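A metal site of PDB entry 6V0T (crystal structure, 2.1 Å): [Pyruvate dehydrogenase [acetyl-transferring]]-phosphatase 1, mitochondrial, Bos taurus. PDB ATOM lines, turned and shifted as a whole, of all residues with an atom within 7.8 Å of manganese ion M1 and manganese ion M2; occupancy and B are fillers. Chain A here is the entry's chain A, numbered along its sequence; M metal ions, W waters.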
ATOM      1  N   ASN A  49       9.686 -34.620  -9.609  1.00  0.00           N
ATOM      2  CA  ASN A  49      11.001 -34.284  -9.117  1.00  0.00           C
ATOM      3  C   ASN A  49      11.491 -35.367  -8.160  1.00  0.00           C
ATOM      4  O   ASN A  49      10.698 -35.964  -7.430  1.00  0.00           O
ATOM      5  CB  ASN A  49      10.990 -32.922  -8.419  1.00  0.00           C
ATOM      6  CG  ASN A  49      10.401 -31.835  -9.281  1.00  0.00           C
ATOM      7  OD1 ASN A  49      11.037 -31.371 -10.228  1.00  0.00           O
ATOM      8  ND2 ASN A  49       9.175 -31.415  -8.971  1.00  0.00           N
ATOM      9  N   ILE A  52      10.195 -35.209  -4.130  1.00  0.00           N
ATOM     10  CA  ILE A  52       8.915 -34.605  -4.477  1.00  0.00           C
ATOM     11  C   ILE A  52       8.714 -33.334  -3.676  1.00  0.00           C
ATOM     12  O   ILE A  52       9.011 -33.267  -2.473  1.00  0.00           O
ATOM     13  CB  ILE A  52       7.764 -35.598  -4.237  1.00  0.00           C
ATOM     14  CG1 ILE A  52       6.487 -35.090  -4.912  1.00  0.00           C
ATOM     15  CG2 ILE A  52       7.530 -35.798  -2.751  1.00  0.00           C
ATOM     16  CD1 ILE A  52       5.373 -36.106  -4.980  1.00  0.00           C
ATOM     17  N   GLU A  53       8.209 -32.292  -4.348  1.00  0.00           N
ATOM     18  CA  GLU A  53       7.973 -31.004  -3.710  1.00  0.00           C
ATOM     19  C   GLU A  53       6.513 -30.764  -3.357  1.00  0.00           C
ATOM     20  O   GLU A  53       6.211 -29.765  -2.708  1.00  0.00           O
ATOM     21  CB  GLU A  53       8.498 -29.881  -4.630  1.00  0.00           C
ATOM     22  CG  GLU A  53       9.998 -29.999  -4.879  1.00  0.00           C
ATOM     23  CD  GLU A  53      10.568 -28.868  -5.726  1.00  0.00           C
ATOM     24  OE1 GLU A  53       9.781 -28.116  -6.336  1.00  0.00           O
ATOM     25  OE2 GLU A  53      11.807 -28.737  -5.763  1.00  0.00           O
ATOM     26  N   ASP A  54       5.619 -31.665  -3.749  1.00  0.00           N
ATOM     27  CA  ASP A  54       4.241 -31.640  -3.283  1.00  0.00           C
ATOM     28  C   ASP A  54       4.151 -32.243  -1.879  1.00  0.00           C
ATOM     29  O   ASP A  54       4.995 -33.029  -1.457  1.00  0.00           O
ATOM     30  CB  ASP A  54       3.330 -32.434  -4.219  1.00  0.00           C
ATOM     31  CG  ASP A  54       2.822 -31.606  -5.386  1.00  0.00           C
ATOM     32  OD1 ASP A  54       3.322 -30.494  -5.609  1.00  0.00           O
ATOM     33  OD2 ASP A  54       1.915 -32.104  -6.087  1.00  0.00           O
ATOM     34  N   PHE A  72      -0.348 -29.042  -0.822  1.00  0.00           N
ATOM     35  CA  PHE A  72       0.632 -27.969  -0.807  1.00  0.00           C
ATOM     36  C   PHE A  72       1.620 -28.203  -1.934  1.00  0.00           C
ATOM     37  O   PHE A  72       2.264 -29.255  -1.991  1.00  0.00           O
ATOM     38  CB  PHE A  72       1.365 -27.909   0.540  1.00  0.00           C
ATOM     39  CG  PHE A  72       0.454 -28.084   1.727  1.00  0.00           C
ATOM     40  CD1 PHE A  72       0.080 -29.358   2.161  1.00  0.00           C
ATOM     41  CD2 PHE A  72      -0.041 -26.993   2.403  1.00  0.00           C
ATOM     42  CE1 PHE A  72      -0.756 -29.512   3.242  1.00  0.00           C
ATOM     43  CE2 PHE A  72      -0.884 -27.144   3.490  1.00  0.00           C
ATOM     44  CZ  PHE A  72      -1.239 -28.412   3.909  1.00  0.00           C
ATOM     45  N   ASP A  73       1.730 -27.230  -2.840  1.00  0.00           N
ATOM     46  CA  ASP A  73       2.619 -27.335  -3.998  1.00  0.00           C
ATOM     47  C   ASP A  73       3.868 -26.511  -3.707  1.00  0.00           C
ATOM     48  O   ASP A  73       3.845 -25.286  -3.790  1.00  0.00           O
ATOM     49  CB  ASP A  73       1.918 -26.856  -5.267  1.00  0.00           C
ATOM     50  CG  ASP A  73       2.727 -27.115  -6.512  1.00  0.00           C
ATOM     51  OD1 ASP A  73       3.973 -27.161  -6.415  1.00  0.00           O
ATOM     52  OD2 ASP A  73       2.123 -27.271  -7.593  1.00  0.00           O
ATOM     53  N   GLY A  74       4.964 -27.208  -3.372  1.00  0.00           N
ATOM     54  CA  GLY A  74       6.207 -26.527  -3.092  1.00  0.00           C
ATOM     55  C   GLY A  74       7.014 -26.246  -4.341  1.00  0.00           C
ATOM     56  O   GLY A  74       6.879 -26.894  -5.374  1.00  0.00           O
ATOM     57  N   HIS A  75       7.885 -25.242  -4.235  1.00  0.00           N
ATOM     58  CA  HIS A  75       8.845 -24.929  -5.281  1.00  0.00           C
ATOM     59  C   HIS A  75      10.124 -24.436  -4.630  1.00  0.00           C
ATOM     60  O   HIS A  75      10.150 -24.068  -3.453  1.00  0.00           O
ATOM     61  CB  HIS A  75       8.309 -23.879  -6.263  1.00  0.00           C
ATOM     62  CG  HIS A  75       7.726 -22.669  -5.617  1.00  0.00           C
ATOM     63  ND1 HIS A  75       6.369 -22.518  -5.392  1.00  0.00           N
ATOM     64  CD2 HIS A  75       8.314 -21.547  -5.128  1.00  0.00           C
ATOM     65  CE1 HIS A  75       6.147 -21.359  -4.801  1.00  0.00           C
ATOM     66  NE2 HIS A  75       7.308 -20.753  -4.623  1.00  0.00           N
ATOM     67  N   ALA A  76      11.206 -24.437  -5.416  1.00  0.00           N
ATOM     68  CA  ALA A  76      12.533 -24.106  -4.906  1.00  0.00           C
ATOM     69  C   ALA A  76      12.909 -25.026  -3.754  1.00  0.00           C
ATOM     70  O   ALA A  76      13.560 -24.621  -2.792  1.00  0.00           O
ATOM     71  CB  ALA A  76      12.610 -22.634  -4.473  1.00  0.00           C
ATOM     72  N   GLY A  77      12.495 -26.291  -3.857  1.00  0.00           N
ATOM     73  CA  GLY A  77      12.719 -27.279  -2.815  1.00  0.00           C
ATOM     74  C   GLY A  77      11.407 -27.693  -2.160  1.00  0.00           C
ATOM     75  O   GLY A  77      10.317 -27.209  -2.502  1.00  0.00           O
ATOM     76  N   SER A  81       7.061 -26.527   1.667  1.00  0.00           N
ATOM     77  CA  SER A  81       5.864 -27.353   1.533  1.00  0.00           C
ATOM     78  C   SER A  81       5.745 -28.319   2.707  1.00  0.00           C
ATOM     79  O   SER A  81       4.667 -28.465   3.285  1.00  0.00           O
ATOM     80  CB  SER A  81       5.879 -28.111   0.201  1.00  0.00           C
ATOM     81  OG  SER A  81       7.066 -28.868   0.055  1.00  0.00           O
ATOM     82  N   GLY A 200       9.187 -21.932  -1.317  1.00  0.00           N
ATOM     83  CA  GLY A 200       7.799 -21.524  -1.286  1.00  0.00           C
ATOM     84  C   GLY A 200       6.861 -22.714  -1.388  1.00  0.00           C
ATOM     85  O   GLY A 200       7.271 -23.818  -1.744  1.00  0.00           O
ATOM     86  N   ALA A 201       5.598 -22.459  -1.082  1.00  0.00           N
ATOM     87  CA  ALA A 201       4.586 -23.507  -1.119  1.00  0.00           C
ATOM     88  C   ALA A 201       3.203 -22.888  -1.224  1.00  0.00           C
ATOM     89  O   ALA A 201       2.875 -21.962  -0.477  1.00  0.00           O
ATOM     90  CB  ALA A 201       4.670 -24.389   0.133  1.00  0.00           C
ATOM     91  N   THR A 202       2.400 -23.417  -2.139  1.00  0.00           N
ATOM     92  CA  THR A 202       0.971 -23.142  -2.136  1.00  0.00           C
ATOM     93  C   THR A 202       0.308 -23.925  -1.000  1.00  0.00           C
ATOM     94  O   THR A 202       0.915 -24.793  -0.367  1.00  0.00           O
ATOM     95  CB  THR A 202       0.325 -23.512  -3.466  1.00  0.00           C
ATOM     96  OG1 THR A 202       0.267 -24.933  -3.602  1.00  0.00           O
ATOM     97  CG2 THR A 202       1.112 -22.923  -4.623  1.00  0.00           C
ATOM     98  N   ASP A 220      -2.055 -21.762  -6.699  1.00  0.00           N
ATOM     99  CA  ASP A 220      -2.673 -22.328  -7.892  1.00  0.00           C
ATOM    100  C   ASP A 220      -3.002 -23.805  -7.757  1.00  0.00           C
ATOM    101  O   ASP A 220      -3.319 -24.456  -8.765  1.00  0.00           O
ATOM    102  CB  ASP A 220      -1.789 -22.096  -9.116  1.00  0.00           C
ATOM    103  CG  ASP A 220      -0.375 -22.626  -8.934  1.00  0.00           C
ATOM    104  OD1 ASP A 220      -0.139 -23.407  -7.980  1.00  0.00           O
ATOM    105  OD2 ASP A 220       0.499 -22.257  -9.738  1.00  0.00           O
ATOM    106  N   SER A 221      -2.933 -24.366  -6.554  1.00  0.00           N
ATOM    107  CA  SER A 221      -3.648 -25.607  -6.278  1.00  0.00           C
ATOM    108  C   SER A 221      -5.143 -25.293  -6.191  1.00  0.00           C
ATOM    109  O   SER A 221      -5.546 -24.140  -6.015  1.00  0.00           O
ATOM    110  CB  SER A 221      -3.145 -26.252  -4.995  1.00  0.00           C
ATOM    111  OG  SER A 221      -1.725 -26.361  -5.002  1.00  0.00           O
ATOM    112  N   THR A 346      -3.027 -30.493  -6.462  1.00  0.00           N
ATOM    113  CA  THR A 346      -2.079 -29.531  -7.008  1.00  0.00           C
ATOM    114  C   THR A 346      -2.297 -29.420  -8.511  1.00  0.00           C
ATOM    115  O   THR A 346      -2.975 -30.235  -9.143  1.00  0.00           O
ATOM    116  CB  THR A 346      -0.655 -29.955  -6.698  1.00  0.00           C
ATOM    117  OG1 THR A 346      -0.418 -31.279  -7.190  1.00  0.00           O
ATOM    118  CG2 THR A 346      -0.406 -29.938  -5.193  1.00  0.00           C
ATOM    119  N   ASP A 347      -1.702 -28.387  -9.109  1.00  0.00           N
ATOM    120  CA  ASP A 347      -1.879 -28.167 -10.535  1.00  0.00           C
ATOM    121  C   ASP A 347      -1.319 -29.310 -11.375  1.00  0.00           C
ATOM    122  O   ASP A 347      -1.596 -29.367 -12.576  1.00  0.00           O
ATOM    123  CB  ASP A 347      -1.229 -26.847 -10.964  1.00  0.00           C
ATOM    124  CG  ASP A 347       0.241 -26.780 -10.637  1.00  0.00           C
ATOM    125  OD1 ASP A 347       0.761 -27.730 -10.001  1.00  0.00           O
ATOM    126  OD2 ASP A 347       0.884 -25.781 -11.009  1.00  0.00           O
ATOM    127  N   GLY A 348      -0.561 -30.230 -10.775  1.00  0.00           N
ATOM    128  CA  GLY A 348      -0.101 -31.388 -11.509  1.00  0.00           C
ATOM    129  C   GLY A 348      -1.229 -32.226 -12.073  1.00  0.00           C
ATOM    130  O   GLY A 348      -1.039 -32.934 -13.061  1.00  0.00           O
ATOM    131  N   LEU A 349      -2.405 -32.156 -11.453  1.00  0.00           N
ATOM    132  CA  LEU A 349      -3.599 -32.797 -11.991  1.00  0.00           C
ATOM    133  C   LEU A 349      -4.370 -31.853 -12.905  1.00  0.00           C
ATOM    134  O   LEU A 349      -4.698 -32.202 -14.036  1.00  0.00           O
ATOM    135  CB  LEU A 349      -4.503 -33.265 -10.850  1.00  0.00           C
ATOM    136  CG  LEU A 349      -5.931 -33.653 -11.249  1.00  0.00           C
ATOM    137  CD1 LEU A 349      -5.919 -34.866 -12.176  1.00  0.00           C
ATOM    138  CD2 LEU A 349      -6.793 -33.935 -10.020  1.00  0.00           C
ATOM    139  N   GLU A 351      -3.666 -29.279 -14.623  1.00  0.00           N
ATOM    140  CA  GLU A 351      -3.070 -29.014 -15.930  1.00  0.00           C
ATOM    141  C   GLU A 351      -3.290 -30.160 -16.905  1.00  0.00           C
ATOM    142  O   GLU A 351      -3.230 -29.943 -18.120  1.00  0.00           O
ATOM    143  CB  GLU A 351      -1.571 -28.738 -15.776  1.00  0.00           C
ATOM    144  CG  GLU A 351      -0.718 -29.978 -15.497  1.00  0.00           C
ATOM    145  CD  GLU A 351       0.772 -29.714 -15.650  1.00  0.00           C
ATOM    146  OE1 GLU A 351       1.571 -30.335 -14.908  1.00  0.00           O
ATOM    147  OE2 GLU A 351       1.144 -28.890 -16.508  1.00  0.00           O
ATOM    148  N   ARG A 441      10.122 -34.951 -15.211  1.00  0.00           N
ATOM    149  CA  ARG A 441       9.635 -33.587 -15.112  1.00  0.00           C
ATOM    150  C   ARG A 441       9.483 -32.913 -16.474  1.00  0.00           C
ATOM    151  O   ARG A 441       8.941 -31.802 -16.528  1.00  0.00           O
ATOM    152  CB  ARG A 441      10.575 -32.761 -14.227  1.00  0.00           C
ATOM    153  CG  ARG A 441      11.972 -32.563 -14.798  1.00  0.00           C
ATOM    154  CD  ARG A 441      12.903 -31.931 -13.775  1.00  0.00           C
ATOM    155  NE  ARG A 441      12.194 -31.021 -12.873  1.00  0.00           N
ATOM    156  CZ  ARG A 441      12.248 -29.689 -12.934  1.00  0.00           C
ATOM    157  NH1 ARG A 441      12.989 -29.077 -13.849  1.00  0.00           N
ATOM    158  NH2 ARG A 441      11.554 -28.957 -12.066  1.00  0.00           N
ATOM    159  N   ASP A 445       4.230 -32.951 -13.989  1.00  0.00           N
ATOM    160  CA  ASP A 445       4.533 -32.263 -12.739  1.00  0.00           C
ATOM    161  C   ASP A 445       4.227 -33.203 -11.582  1.00  0.00           C
ATOM    162  O   ASP A 445       3.590 -34.248 -11.742  1.00  0.00           O
ATOM    163  CB  ASP A 445       3.712 -30.978 -12.649  1.00  0.00           C
ATOM    164  CG  ASP A 445       4.078 -30.117 -11.453  1.00  0.00           C
ATOM    165  OD1 ASP A 445       5.156 -30.337 -10.841  1.00  0.00           O
ATOM    166  OD2 ASP A 445       3.296 -29.206 -11.124  1.00  0.00           O
ATOM    167  N   ASP A 446       4.701 -32.842 -10.387  1.00  0.00           N
ATOM    168  CA  ASP A 446       4.264 -33.517  -9.174  1.00  0.00           C
ATOM    169  C   ASP A 446       2.748 -33.527  -9.136  1.00  0.00           C
ATOM    170  O   ASP A 446       2.101 -32.495  -9.354  1.00  0.00           O
ATOM    171  CB  ASP A 446       4.823 -32.828  -7.936  1.00  0.00           C
ATOM    172  CG  ASP A 446       6.328 -32.921  -7.840  1.00  0.00           C
ATOM    173  OD1 ASP A 446       6.897 -33.920  -8.329  1.00  0.00           O
ATOM    174  OD2 ASP A 446       6.937 -31.991  -7.262  1.00  0.00           O
ATOM    175  N   ILE A 447       2.167 -34.696  -8.863  1.00  0.00           N
ATOM    176  CA  ILE A 447       0.723 -34.877  -8.806  1.00  0.00           C
ATOM    177  C   ILE A 447       0.338 -35.327  -7.408  1.00  0.00           C
ATOM    178  O   ILE A 447       0.875 -36.323  -6.899  1.00  0.00           O
ATOM    179  CB  ILE A 447       0.231 -35.879  -9.857  1.00  0.00           C
ATOM    180  CG1 ILE A 447       0.475 -35.331 -11.270  1.00  0.00           C
ATOM    181  CG2 ILE A 447      -1.263 -36.162  -9.664  1.00  0.00           C
ATOM    182  CD1 ILE A 447       0.399 -36.384 -12.356  1.00  0.00           C
HETATM  183 MN    MN M   1       2.822 -28.003  -9.446  1.00  0.00          MN
HETATM  184 MN    MN M   2       5.893 -27.566  -7.189  1.00  0.00          MN
HETATM  185  O   HOH W   1       2.562 -29.994  -8.436  1.00  0.00           O
HETATM  186  O   HOH W   2       5.973 -25.676  -8.149  1.00  0.00           O
HETATM  187  O   HOH W   3       4.983 -28.082  -9.227  1.00  0.00           O
HETATM  188  O   HOH W   4       5.499 -29.739  -6.393  1.00  0.00           O
HETATM  189  O   HOH W   5       3.142 -26.185 -10.256  1.00  0.00           O
HETATM  190  O   HOH W   6       8.081 -28.118  -7.873  1.00  0.00           O
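The backbone NH (N) of Asp 73 is in hydrogen-bond range of the side-chain hydroxyl (OG1) of Thr 202 (2.8 Å). The backbone carbonyl oxygen of Glu 53 lies within hydrogen-bond range of the backbone NH of Gly 74 (2.9 Å).
Two residues have an atom within 4 Å of manganese ion M2: Asp 73 and Gly 74.
Water W5 binds manganese ion M1 (2.0 Å). Manganese ion M1 is bound by the side-chain carboxylate (OD2) of Asp 73, at 2.1 Å. Manganese ion M1 is bound by the side-chain carboxylate (OD2) of Asp 445, at 2.1 Å. OD1 of Asp 347 is bound to manganese ion M1 (2.2 Å). Water W3 binds manganese ion M1 (2.2 Å). Water W1 binds manganese ion M1 (2.2 Å).
Manganese ion M2 is bound by the side-chain carboxylate of Asp 73 (2.1 Å), water W2 (2.1 Å), the backbone carbonyl oxygen of Gly 74 (2.2 Å), water W3 (2.3 Å), water W4 (2.3 Å) and water W6 (2.4 Å). Manganese ion M2 has six donor atoms within binding distance.
Water W1 lies within hydrogen-bond range of the backbone carbonyl oxygen of Asp 446 (2.7 Å), the side-chain carboxylate of Asp 54 (3.0 Å) and the side-chain hydroxyl of Thr 346 (3.5 Å). Water W4 lies within hydrogen-bond range of OD1 of Asp 54 (2.4 Å) and OD2 of Asp 446 (2.8 Å).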
